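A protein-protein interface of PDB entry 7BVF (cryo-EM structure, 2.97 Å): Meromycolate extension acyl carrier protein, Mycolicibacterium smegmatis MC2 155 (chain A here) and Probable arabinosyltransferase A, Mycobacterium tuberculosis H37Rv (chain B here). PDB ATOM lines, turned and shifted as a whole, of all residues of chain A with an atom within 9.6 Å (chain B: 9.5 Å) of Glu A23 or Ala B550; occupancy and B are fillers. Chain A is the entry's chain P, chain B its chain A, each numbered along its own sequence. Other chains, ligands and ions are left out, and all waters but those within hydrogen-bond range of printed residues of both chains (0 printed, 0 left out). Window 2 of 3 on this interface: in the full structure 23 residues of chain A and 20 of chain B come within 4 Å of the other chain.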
ATOM      1  N   ILE A   9     -19.672  26.443 -24.619  1.00  0.00           N
ATOM      2  CA  ILE A   9     -18.602  26.833 -23.710  1.00  0.00           C
ATOM      3  C   ILE A   9     -18.024  25.586 -23.058  1.00  0.00           C
ATOM      4  O   ILE A   9     -16.824  25.521 -22.780  1.00  0.00           O
ATOM      5  CB  ILE A   9     -19.099  27.843 -22.662  1.00  0.00           C
ATOM      6  CG1 ILE A   9     -19.566  29.125 -23.354  1.00  0.00           C
ATOM      7  CG2 ILE A   9     -18.005  28.161 -21.661  1.00  0.00           C
ATOM      8  CD1 ILE A   9     -19.655  30.327 -22.436  1.00  0.00           C
ATOM      9  N   LEU A  12     -15.452  24.389 -25.587  1.00  0.00           N
ATOM     10  CA  LEU A  12     -14.455  25.407 -25.895  1.00  0.00           C
ATOM     11  C   LEU A  12     -13.506  25.618 -24.723  1.00  0.00           C
ATOM     12  O   LEU A  12     -12.295  25.760 -24.921  1.00  0.00           O
ATOM     13  CB  LEU A  12     -15.138  26.719 -26.276  1.00  0.00           C
ATOM     14  CG  LEU A  12     -15.432  26.929 -27.761  1.00  0.00           C
ATOM     15  CD1 LEU A  12     -14.132  27.034 -28.537  1.00  0.00           C
ATOM     16  CD2 LEU A  12     -16.312  25.827 -28.329  1.00  0.00           C
ATOM     17  N   ALA A  13     -14.030  25.635 -23.496  1.00  0.00           N
ATOM     18  CA  ALA A  13     -13.188  25.777 -22.317  1.00  0.00           C
ATOM     19  C   ALA A  13     -12.364  24.532 -22.032  1.00  0.00           C
ATOM     20  O   ALA A  13     -11.485  24.579 -21.169  1.00  0.00           O
ATOM     21  CB  ALA A  13     -14.043  26.116 -21.101  1.00  0.00           C
ATOM     22  N   GLU A  14     -12.632  23.425 -22.718  1.00  0.00           N
ATOM     23  CA  GLU A  14     -11.790  22.240 -22.651  1.00  0.00           C
ATOM     24  C   GLU A  14     -10.724  22.234 -23.736  1.00  0.00           C
ATOM     25  O   GLU A  14      -9.574  21.878 -23.471  1.00  0.00           O
ATOM     26  CB  GLU A  14     -12.646  20.975 -22.767  1.00  0.00           C
ATOM     27  CG  GLU A  14     -11.899  19.645 -22.627  1.00  0.00           C
ATOM     28  CD  GLU A  14     -11.019  19.554 -21.388  1.00  0.00           C
ATOM     29  OE1 GLU A  14      -9.941  20.183 -21.351  1.00  0.00           O
ATOM     30  OE2 GLU A  14     -11.412  18.838 -20.441  1.00  0.00           O
ATOM     31  N   ILE A  15     -11.082  22.651 -24.951  1.00  0.00           N
ATOM     32  CA  ILE A  15     -10.096  22.786 -26.020  1.00  0.00           C
ATOM     33  C   ILE A  15      -9.061  23.844 -25.659  1.00  0.00           C
ATOM     34  O   ILE A  15      -7.856  23.653 -25.866  1.00  0.00           O
ATOM     35  CB  ILE A  15     -10.798  23.110 -27.351  1.00  0.00           C
ATOM     36  CG1 ILE A  15     -11.625  21.915 -27.822  1.00  0.00           C
ATOM     37  CG2 ILE A  15      -9.787  23.501 -28.409  1.00  0.00           C
ATOM     38  CD1 ILE A  15     -12.526  22.226 -28.986  1.00  0.00           C
ATOM     39  N   ILE A  16      -9.511  24.972 -25.106  1.00  0.00           N
ATOM     40  CA  ILE A  16      -8.588  26.040 -24.735  1.00  0.00           C
ATOM     41  C   ILE A  16      -7.652  25.577 -23.628  1.00  0.00           C
ATOM     42  O   ILE A  16      -6.455  25.878 -23.645  1.00  0.00           O
ATOM     43  CB  ILE A  16      -9.371  27.302 -24.331  1.00  0.00           C
ATOM     44  CG1 ILE A  16     -10.028  27.935 -25.555  1.00  0.00           C
ATOM     45  CG2 ILE A  16      -8.464  28.307 -23.657  1.00  0.00           C
ATOM     46  CD1 ILE A  16     -10.673  29.265 -25.275  1.00  0.00           C
ATOM     47  N   GLU A  17      -8.175  24.835 -22.651  1.00  0.00           N
ATOM     48  CA  GLU A  17      -7.317  24.307 -21.596  1.00  0.00           C
ATOM     49  C   GLU A  17      -6.319  23.298 -22.143  1.00  0.00           C
ATOM     50  O   GLU A  17      -5.163  23.263 -21.711  1.00  0.00           O
ATOM     51  CB  GLU A  17      -8.161  23.669 -20.496  1.00  0.00           C
ATOM     52  CG  GLU A  17      -7.385  23.380 -19.224  1.00  0.00           C
ATOM     53  CD  GLU A  17      -7.904  22.163 -18.481  1.00  0.00           C
ATOM     54  OE1 GLU A  17      -9.129  22.077 -18.257  1.00  0.00           O
ATOM     55  OE2 GLU A  17      -7.084  21.292 -18.118  1.00  0.00           O
ATOM     56  N   GLU A  18      -6.748  22.460 -23.087  1.00  0.00           N
ATOM     57  CA  GLU A  18      -5.848  21.459 -23.645  1.00  0.00           C
ATOM     58  C   GLU A  18      -4.764  22.091 -24.506  1.00  0.00           C
ATOM     59  O   GLU A  18      -3.666  21.536 -24.621  1.00  0.00           O
ATOM     60  CB  GLU A  18      -6.643  20.441 -24.461  1.00  0.00           C
ATOM     61  CG  GLU A  18      -5.944  19.110 -24.656  1.00  0.00           C
ATOM     62  CD  GLU A  18      -6.813  18.101 -25.379  1.00  0.00           C
ATOM     63  OE1 GLU A  18      -7.882  18.494 -25.892  1.00  0.00           O
ATOM     64  OE2 GLU A  18      -6.430  16.913 -25.433  1.00  0.00           O
ATOM     65  N   VAL A  19      -5.048  23.238 -25.114  1.00  0.00           N
ATOM     66  CA  VAL A  19      -4.090  23.865 -26.021  1.00  0.00           C
ATOM     67  C   VAL A  19      -3.157  24.824 -25.290  1.00  0.00           C
ATOM     68  O   VAL A  19      -1.943  24.788 -25.496  1.00  0.00           O
ATOM     69  CB  VAL A  19      -4.845  24.570 -27.163  1.00  0.00           C
ATOM     70  CG1 VAL A  19      -3.944  25.548 -27.872  1.00  0.00           C
ATOM     71  CG2 VAL A  19      -5.383  23.546 -28.139  1.00  0.00           C
ATOM     72  N   THR A  20      -3.683  25.688 -24.423  1.00  0.00           N
ATOM     73  CA  THR A  20      -2.879  26.730 -23.802  1.00  0.00           C
ATOM     74  C   THR A  20      -2.606  26.510 -22.322  1.00  0.00           C
ATOM     75  O   THR A  20      -1.800  27.246 -21.746  1.00  0.00           O
ATOM     76  CB  THR A  20      -3.558  28.096 -23.970  1.00  0.00           C
ATOM     77  OG1 THR A  20      -4.610  28.223 -23.012  1.00  0.00           O
ATOM     78  CG2 THR A  20      -4.140  28.232 -25.359  1.00  0.00           C
ATOM     79  N   GLY A  21      -3.243  25.531 -21.690  1.00  0.00           N
ATOM     80  CA  GLY A  21      -3.115  25.362 -20.260  1.00  0.00           C
ATOM     81  C   GLY A  21      -3.942  26.316 -19.429  1.00  0.00           C
ATOM     82  O   GLY A  21      -3.912  26.219 -18.197  1.00  0.00           O
ATOM     83  N   ILE A  22      -4.673  27.234 -20.061  1.00  0.00           N
ATOM     84  CA  ILE A  22      -5.512  28.174 -19.330  1.00  0.00           C
ATOM     85  C   ILE A  22      -6.653  27.420 -18.664  1.00  0.00           C
ATOM     86  O   ILE A  22      -7.335  26.607 -19.298  1.00  0.00           O
ATOM     87  CB  ILE A  22      -6.035  29.265 -20.273  1.00  0.00           C
ATOM     88  CG1 ILE A  22      -4.922  30.265 -20.590  1.00  0.00           C
ATOM     89  CG2 ILE A  22      -7.228  29.975 -19.667  1.00  0.00           C
ATOM     90  CD1 ILE A  22      -5.283  31.266 -21.654  1.00  0.00           C
ATOM     91  N   GLU A  23      -6.869  27.692 -17.382  1.00  0.00           N
ATOM     92  CA  GLU A  23      -7.865  26.957 -16.621  1.00  0.00           C
ATOM     93  C   GLU A  23      -9.267  27.254 -17.147  1.00  0.00           C
ATOM     94  O   GLU A  23      -9.558  28.389 -17.536  1.00  0.00           O
ATOM     95  CB  GLU A  23      -7.773  27.324 -15.144  1.00  0.00           C
ATOM     96  CG  GLU A  23      -6.475  26.897 -14.493  1.00  0.00           C
ATOM     97  CD  GLU A  23      -6.385  27.331 -13.048  1.00  0.00           C
ATOM     98  OE1 GLU A  23      -7.280  28.074 -12.593  1.00  0.00           O
ATOM     99  OE2 GLU A  23      -5.419  26.932 -12.365  1.00  0.00           O
ATOM    100  N   PRO A  24     -10.160  26.260 -17.170  1.00  0.00           N
ATOM    101  CA  PRO A  24     -11.525  26.513 -17.653  1.00  0.00           C
ATOM    102  C   PRO A  24     -12.341  27.399 -16.732  1.00  0.00           C
ATOM    103  O   PRO A  24     -13.382  27.910 -17.160  1.00  0.00           O
ATOM    104  CB  PRO A  24     -12.129  25.107 -17.748  1.00  0.00           C
ATOM    105  CG  PRO A  24     -11.364  24.309 -16.754  1.00  0.00           C
ATOM    106  CD  PRO A  24      -9.966  24.858 -16.764  1.00  0.00           C
ATOM    107  N   SER A  25     -11.908  27.594 -15.485  1.00  0.00           N
ATOM    108  CA  SER A  25     -12.622  28.482 -14.575  1.00  0.00           C
ATOM    109  C   SER A  25     -12.662  29.914 -15.086  1.00  0.00           C
ATOM    110  O   SER A  25     -13.564  30.669 -14.712  1.00  0.00           O
ATOM    111  CB  SER A  25     -11.973  28.446 -13.191  1.00  0.00           C
ATOM    112  OG  SER A  25     -12.060  27.154 -12.618  1.00  0.00           O
ATOM    113  N   GLU A  26     -11.714  30.299 -15.933  1.00  0.00           N
ATOM    114  CA  GLU A  26     -11.605  31.651 -16.460  1.00  0.00           C
ATOM    115  C   GLU A  26     -11.819  31.669 -17.969  1.00  0.00           C
ATOM    116  O   GLU A  26     -11.083  32.315 -18.716  1.00  0.00           O
ATOM    117  CB  GLU A  26     -10.261  32.270 -16.079  1.00  0.00           C
ATOM    118  CG  GLU A  26      -9.043  31.524 -16.603  1.00  0.00           C
ATOM    119  CD  GLU A  26      -7.741  32.141 -16.134  1.00  0.00           C
ATOM    120  OE1 GLU A  26      -7.792  33.137 -15.384  1.00  0.00           O
ATOM    121  OE2 GLU A  26      -6.667  31.629 -16.513  1.00  0.00           O
ATOM    122  N   VAL A  27     -12.829  30.945 -18.435  1.00  0.00           N
ATOM    123  CA  VAL A  27     -13.256  30.984 -19.833  1.00  0.00           C
ATOM    124  C   VAL A  27     -14.737  31.343 -19.817  1.00  0.00           C
ATOM    125  O   VAL A  27     -15.611  30.480 -19.701  1.00  0.00           O
ATOM    126  CB  VAL A  27     -12.999  29.664 -20.566  1.00  0.00           C
ATOM    127  CG1 VAL A  27     -13.539  29.734 -21.983  1.00  0.00           C
ATOM    128  CG2 VAL A  27     -11.514  29.350 -20.581  1.00  0.00           C
ATOM    129  N   THR A  28     -15.028  32.636 -19.926  1.00  0.00           N
ATOM    130  CA  THR A  28     -16.373  33.179 -19.868  1.00  0.00           C
ATOM    131  C   THR A  28     -16.607  34.075 -21.076  1.00  0.00           C
ATOM    132  O   THR A  28     -15.663  34.676 -21.597  1.00  0.00           O
ATOM    133  CB  THR A  28     -16.592  33.975 -18.572  1.00  0.00           C
ATOM    134  OG1 THR A  28     -15.754  35.136 -18.570  1.00  0.00           O
ATOM    135  CG2 THR A  28     -16.273  33.119 -17.354  1.00  0.00           C
ATOM    136  N   LYS A  31     -14.890  38.090 -22.369  1.00  0.00           N
ATOM    137  CA  LYS A  31     -13.512  38.533 -22.525  1.00  0.00           C
ATOM    138  C   LYS A  31     -12.941  38.064 -23.855  1.00  0.00           C
ATOM    139  O   LYS A  31     -13.230  36.954 -24.312  1.00  0.00           O
ATOM    140  CB  LYS A  31     -12.642  38.022 -21.377  1.00  0.00           C
ATOM    141  CG  LYS A  31     -12.880  36.571 -21.031  1.00  0.00           C
ATOM    142  CD  LYS A  31     -12.517  36.304 -19.590  1.00  0.00           C
ATOM    143  CE  LYS A  31     -12.706  34.849 -19.250  1.00  0.00           C
ATOM    144  NZ  LYS A  31     -11.858  33.988 -20.117  1.00  0.00           N
ATOM    145  N   LEU A  37      -7.097  36.940 -22.191  1.00  0.00           N
ATOM    146  CA  LEU A  37      -6.209  35.824 -22.458  1.00  0.00           C
ATOM    147  C   LEU A  37      -5.000  36.308 -23.257  1.00  0.00           C
ATOM    148  O   LEU A  37      -4.892  37.476 -23.638  1.00  0.00           O
ATOM    149  CB  LEU A  37      -6.958  34.721 -23.200  1.00  0.00           C
ATOM    150  CG  LEU A  37      -8.376  34.433 -22.710  1.00  0.00           C
ATOM    151  CD1 LEU A  37      -9.085  33.477 -23.649  1.00  0.00           C
ATOM    152  CD2 LEU A  37      -8.347  33.874 -21.304  1.00  0.00           C
ATOM    153  N   GLY B 356       2.784  26.589 -22.413  1.00  0.00           N
ATOM    154  CA  GLY B 356       2.139  27.579 -21.584  1.00  0.00           C
ATOM    155  C   GLY B 356       2.142  28.987 -22.150  1.00  0.00           C
ATOM    156  O   GLY B 356       2.797  29.887 -21.620  1.00  0.00           O
ATOM    157  N   GLY B 358       0.100  31.736 -21.979  1.00  0.00           N
ATOM    158  CA  GLY B 358      -1.039  32.411 -21.407  1.00  0.00           C
ATOM    159  C   GLY B 358      -0.680  33.367 -20.291  1.00  0.00           C
ATOM    160  O   GLY B 358       0.492  33.659 -20.043  1.00  0.00           O
ATOM    161  N   PRO B 359      -1.696  33.879 -19.593  1.00  0.00           N
ATOM    162  CA  PRO B 359      -1.458  34.720 -18.416  1.00  0.00           C
ATOM    163  C   PRO B 359      -0.949  33.964 -17.200  1.00  0.00           C
ATOM    164  O   PRO B 359      -0.912  34.538 -16.108  1.00  0.00           O
ATOM    165  CB  PRO B 359      -2.849  35.318 -18.134  1.00  0.00           C
ATOM    166  CG  PRO B 359      -3.668  35.040 -19.352  1.00  0.00           C
ATOM    167  CD  PRO B 359      -3.128  33.771 -19.906  1.00  0.00           C
ATOM    168  N   GLY B 360      -0.552  32.708 -17.367  1.00  0.00           N
ATOM    169  CA  GLY B 360      -0.082  31.891 -16.273  1.00  0.00           C
ATOM    170  C   GLY B 360       1.425  31.925 -16.177  1.00  0.00           C
ATOM    171  O   GLY B 360       1.989  32.919 -15.715  1.00  0.00           O
ATOM    172  N   GLY B 361       2.097  30.860 -16.610  1.00  0.00           N
ATOM    173  CA  GLY B 361       3.523  30.745 -16.395  1.00  0.00           C
ATOM    174  C   GLY B 361       4.252  30.139 -17.576  1.00  0.00           C
ATOM    175  O   GLY B 361       3.669  29.859 -18.623  1.00  0.00           O
ATOM    176  N   LEU B 362       5.562  29.975 -17.378  1.00  0.00           N
ATOM    177  CA  LEU B 362       6.517  29.418 -18.330  1.00  0.00           C
ATOM    178  C   LEU B 362       6.739  30.349 -19.514  1.00  0.00           C
ATOM    179  O   LEU B 362       7.571  30.073 -20.382  1.00  0.00           O
ATOM    180  CB  LEU B 362       6.082  28.034 -18.808  1.00  0.00           C
ATOM    181  CG  LEU B 362       7.271  27.164 -19.209  1.00  0.00           C
ATOM    182  CD1 LEU B 362       8.350  27.244 -18.158  1.00  0.00           C
ATOM    183  CD2 LEU B 362       6.845  25.744 -19.405  1.00  0.00           C
ATOM    184  N   VAL B 542       5.593  14.041 -11.665  1.00  0.00           N
ATOM    185  CA  VAL B 542       4.542  15.034 -11.460  1.00  0.00           C
ATOM    186  C   VAL B 542       3.531  15.029 -12.603  1.00  0.00           C
ATOM    187  O   VAL B 542       2.432  15.573 -12.458  1.00  0.00           O
ATOM    188  CB  VAL B 542       5.177  16.423 -11.259  1.00  0.00           C
ATOM    189  CG1 VAL B 542       4.130  17.476 -10.969  1.00  0.00           C
ATOM    190  CG2 VAL B 542       6.168  16.375 -10.120  1.00  0.00           C
ATOM    191  N   LEU B 543       3.865  14.429 -13.742  1.00  0.00           N
ATOM    192  CA  LEU B 543       2.889  14.278 -14.813  1.00  0.00           C
ATOM    193  C   LEU B 543       2.110  12.978 -14.710  1.00  0.00           C
ATOM    194  O   LEU B 543       0.934  12.942 -15.086  1.00  0.00           O
ATOM    195  CB  LEU B 543       3.579  14.345 -16.177  1.00  0.00           C
ATOM    196  CG  LEU B 543       3.827  15.725 -16.783  1.00  0.00           C
ATOM    197  CD1 LEU B 543       4.601  15.586 -18.075  1.00  0.00           C
ATOM    198  CD2 LEU B 543       2.521  16.447 -17.022  1.00  0.00           C
ATOM    199  N   ARG B 546      -1.324  13.339 -10.696  1.00  0.00           N
ATOM    200  CA  ARG B 546      -1.915  14.651 -11.078  1.00  0.00           C
ATOM    201  C   ARG B 546      -1.556  14.903 -12.549  1.00  0.00           C
ATOM    202  O   ARG B 546      -0.471  15.461 -12.806  1.00  0.00           O
ATOM    203  CB  ARG B 546      -1.377  15.765 -10.175  1.00  0.00           C
ATOM    204  CG  ARG B 546       0.048  15.538  -9.690  1.00  0.00           C
ATOM    205  CD  ARG B 546       0.365  16.331  -8.436  1.00  0.00           C
ATOM    206  NE  ARG B 546      -0.235  17.657  -8.452  1.00  0.00           N
ATOM    207  CZ  ARG B 546      -0.248  18.490  -7.418  1.00  0.00           C
ATOM    208  NH1 ARG B 546       0.310  18.134  -6.273  1.00  0.00           N
ATOM    209  NH2 ARG B 546      -0.818  19.677  -7.531  1.00  0.00           N
ATOM    210  N   GLY B 547      -2.463  14.573 -13.440  1.00  0.00           N
ATOM    211  CA  GLY B 547      -2.184  14.640 -14.878  1.00  0.00           C
ATOM    212  C   GLY B 547      -1.974  16.039 -15.388  1.00  0.00           C
ATOM    213  O   GLY B 547      -1.482  16.179 -16.482  1.00  0.00           O
ATOM    214  N   ARG B 548      -2.410  17.041 -14.644  1.00  0.00           N
ATOM    215  CA  ARG B 548      -2.328  18.411 -15.133  1.00  0.00           C
ATOM    216  C   ARG B 548      -1.271  19.196 -14.362  1.00  0.00           C
ATOM    217  O   ARG B 548      -0.739  18.746 -13.346  1.00  0.00           O
ATOM    218  CB  ARG B 548      -3.686  19.108 -15.022  1.00  0.00           C
ATOM    219  CG  ARG B 548      -4.722  18.623 -16.010  1.00  0.00           C
ATOM    220  CD  ARG B 548      -4.142  18.501 -17.405  1.00  0.00           C
ATOM    221  NE  ARG B 548      -5.168  18.629 -18.436  1.00  0.00           N
ATOM    222  CZ  ARG B 548      -5.041  18.169 -19.676  1.00  0.00           C
ATOM    223  NH1 ARG B 548      -3.932  17.543 -20.040  1.00  0.00           N
ATOM    224  NH2 ARG B 548      -6.024  18.328 -20.550  1.00  0.00           N
ATOM    225  N   VAL B 549      -0.967  20.392 -14.862  1.00  0.00           N
ATOM    226  CA  VAL B 549      -0.004  21.266 -14.200  1.00  0.00           C
ATOM    227  C   VAL B 549      -0.628  22.646 -14.028  1.00  0.00           C
ATOM    228  O   VAL B 549      -0.190  23.438 -13.186  1.00  0.00           O
ATOM    229  CB  VAL B 549       1.324  21.318 -14.979  1.00  0.00           C
ATOM    230  CG1 VAL B 549       2.278  22.344 -14.390  1.00  0.00           C
ATOM    231  CG2 VAL B 549       1.979  19.947 -14.986  1.00  0.00           C
ATOM    232  N   ALA B 550      -1.683  22.928 -14.794  1.00  0.00           N
ATOM    233  CA  ALA B 550      -2.476  24.149 -14.640  1.00  0.00           C
ATOM    234  C   ALA B 550      -1.608  25.399 -14.818  1.00  0.00           C
ATOM    235  O   ALA B 550      -1.385  26.186 -13.899  1.00  0.00           O
ATOM    236  CB  ALA B 550      -3.198  24.162 -13.287  1.00  0.00           C
ATOM    237  N   GLY B 551      -1.118  25.549 -16.044  1.00  0.00           N
ATOM    238  CA  GLY B 551      -0.238  26.643 -16.397  1.00  0.00           C
ATOM    239  C   GLY B 551       0.778  26.198 -17.422  1.00  0.00           C
ATOM    240  O   GLY B 551       1.638  26.971 -17.849  1.00  0.00           O
ATOM    241  N   LEU B 552       0.670  24.938 -17.830  1.00  0.00           N
ATOM    242  CA  LEU B 552       1.619  24.312 -18.739  1.00  0.00           C
ATOM    243  C   LEU B 552       0.858  23.362 -19.647  1.00  0.00           C
ATOM    244  O   LEU B 552       0.168  22.463 -19.158  1.00  0.00           O
ATOM    245  CB  LEU B 552       2.703  23.574 -17.951  1.00  0.00           C
ATOM    246  CG  LEU B 552       3.733  22.710 -18.665  1.00  0.00           C
ATOM    247  CD1 LEU B 552       5.091  22.984 -18.089  1.00  0.00           C
ATOM    248  CD2 LEU B 552       3.379  21.258 -18.465  1.00  0.00           C
ATOM    249  N   ALA B 553       0.971  23.564 -20.957  1.00  0.00           N
ATOM    250  CA  ALA B 553       0.299  22.694 -21.910  1.00  0.00           C
ATOM    251  C   ALA B 553       0.860  21.282 -21.825  1.00  0.00           C
ATOM    252  O   ALA B 553       2.074  21.087 -21.724  1.00  0.00           O
ATOM    253  CB  ALA B 553       0.451  23.238 -23.325  1.00  0.00           C
ATOM    254  N   SER B 554      -0.029  20.292 -21.881  1.00  0.00           N
ATOM    255  CA  SER B 554       0.359  18.914 -21.608  1.00  0.00           C
ATOM    256  C   SER B 554       0.781  18.143 -22.848  1.00  0.00           C
ATOM    257  O   SER B 554       1.581  17.210 -22.736  1.00  0.00           O
ATOM    258  CB  SER B 554      -0.783  18.171 -20.915  1.00  0.00           C
ATOM    259  OG  SER B 554      -1.030  18.715 -19.632  1.00  0.00           O
ATOM    260  N   PHE B 598       9.320  25.533 -12.855  1.00  0.00           N
ATOM    261  CA  PHE B 598       7.944  26.012 -12.833  1.00  0.00           C
ATOM    262  C   PHE B 598       7.028  25.090 -12.037  1.00  0.00           C
ATOM    263  O   PHE B 598       6.198  25.568 -11.259  1.00  0.00           O
ATOM    264  CB  PHE B 598       7.419  26.176 -14.256  1.00  0.00           C
ATOM    265  CG  PHE B 598       6.013  26.681 -14.320  1.00  0.00           C
ATOM    266  CD1 PHE B 598       5.720  27.984 -13.981  1.00  0.00           C
ATOM    267  CD2 PHE B 598       4.984  25.851 -14.717  1.00  0.00           C
ATOM    268  CE1 PHE B 598       4.432  28.449 -14.034  1.00  0.00           C
ATOM    269  CE2 PHE B 598       3.693  26.314 -14.773  1.00  0.00           C
ATOM    270  CZ  PHE B 598       3.418  27.614 -14.431  1.00  0.00           C
ATOM    271  N   THR B 599       7.153  23.771 -12.212  1.00  0.00           N
ATOM    272  CA  THR B 599       6.233  22.859 -11.533  1.00  0.00           C
ATOM    273  C   THR B 599       6.515  22.795 -10.037  1.00  0.00           C
ATOM    274  O   THR B 599       5.604  22.983  -9.219  1.00  0.00           O
ATOM    275  CB  THR B 599       6.294  21.460 -12.144  1.00  0.00           C
ATOM    276  OG1 THR B 599       7.548  20.847 -11.829  1.00  0.00           O
ATOM    277  CG2 THR B 599       6.102  21.510 -13.646  1.00  0.00           C
ATOM    278  N   ARG B 602       4.882  25.391  -7.652  1.00  0.00           N
ATOM    279  CA  ARG B 602       3.473  25.354  -7.289  1.00  0.00           C
ATOM    280  C   ARG B 602       3.057  24.065  -6.609  1.00  0.00           C
ATOM    281  O   ARG B 602       2.133  24.088  -5.799  1.00  0.00           O
ATOM    282  CB  ARG B 602       2.591  25.569  -8.524  1.00  0.00           C
ATOM    283  CG  ARG B 602       2.956  24.704  -9.712  1.00  0.00           C
ATOM    284  CD  ARG B 602       2.101  25.042 -10.916  1.00  0.00           C
ATOM    285  NE  ARG B 602       2.131  26.469 -11.217  1.00  0.00           N
ATOM    286  CZ  ARG B 602       1.086  27.280 -11.095  1.00  0.00           C
ATOM    287  NH1 ARG B 602      -0.078  26.802 -10.681  1.00  0.00           N
ATOM    288  NH2 ARG B 602       1.206  28.566 -11.390  1.00  0.00           N
ATOM    289  N   ILE B 603       3.706  22.936  -6.912  1.00  0.00           N
ATOM    290  CA  ILE B 603       3.392  21.731  -6.145  1.00  0.00           C
ATOM    291  C   ILE B 603       4.143  21.694  -4.827  1.00  0.00           C
ATOM    292  O   ILE B 603       3.825  20.864  -3.968  1.00  0.00           O
ATOM    293  CB  ILE B 603       3.688  20.414  -6.884  1.00  0.00           C
ATOM    294  CG1 ILE B 603       5.186  20.174  -6.999  1.00  0.00           C
ATOM    295  CG2 ILE B 603       3.063  20.427  -8.264  1.00  0.00           C
ATOM    296  CD1 ILE B 603       5.511  18.771  -7.417  1.00  0.00           C
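Among the printed residues, merely in contact across the chains: Val A19 with Ala B553, Thr A20 with Gly B356, Gly A21 with Gly B551, Ile A22 with Pro B359 and Glu A23 with Ala B550.
OG of Ser B554 is in hydrogen-bond range of NH1 of Arg B548, 3.2 Å away.
The side-chain hydroxyl (OG1) of Thr A20 lies within hydrogen-bond range of the backbone carbonyl oxygen (O) of Ile A16, at 3.1 Å.
The side-chain hydroxyl of Thr A20 sits at hydrogen-bond distance from the backbone NH of Ile A22 (3.1 Å).
Of the 21 printed residues of chain B, 6 touch a printed residue of chain A.
Hydrophobic or aromatic side chains of chain B that line the printed part of chain A: Pro B359, Ala B550 and Ala B553.
Among the printed residues, 6 pairs touch across the chains.
Among the printed residues, Asp or Glu carboxylates within 4 Å of a Lys or Arg side-chain nitrogen of the other chain: Glu A17 with Arg B548.
Printed residues of chain B within 4 Å of Val A19: Ala B553.
Of the printed residues of chain B, Ile A22 touches Pro B359.
Of chain B, only Ala B550 (3.7 Å) comes within 4 Å of Glu A23.
Ser A25 touches none of the printed residues of chain B.
Of the printed residues of chain A, Gly B356 touches Thr A20.
Leu B362 touches none of the printed residues of chain A.
Arg B546 touches none of the printed residues of chain A.
No residue of chain A comes within 4 Å of Val B549.
Ala B550 touches one residue of chain A.
Of chain A, only Gly A21 (3.6 Å) comes within 4 Å of Gly B551.
The nearest residue of chain B that does not touch Glu A23 is Arg B602 (5.6 Å).
The nearest printed residue of chain A that does not touch Pro B359 is Leu A37 (4.1 Å).
The side-chain carboxylate (OE2) of Glu A17 is in salt-bridge range of the guanidinium group (NE) of Arg B548, 3.3 Å away.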
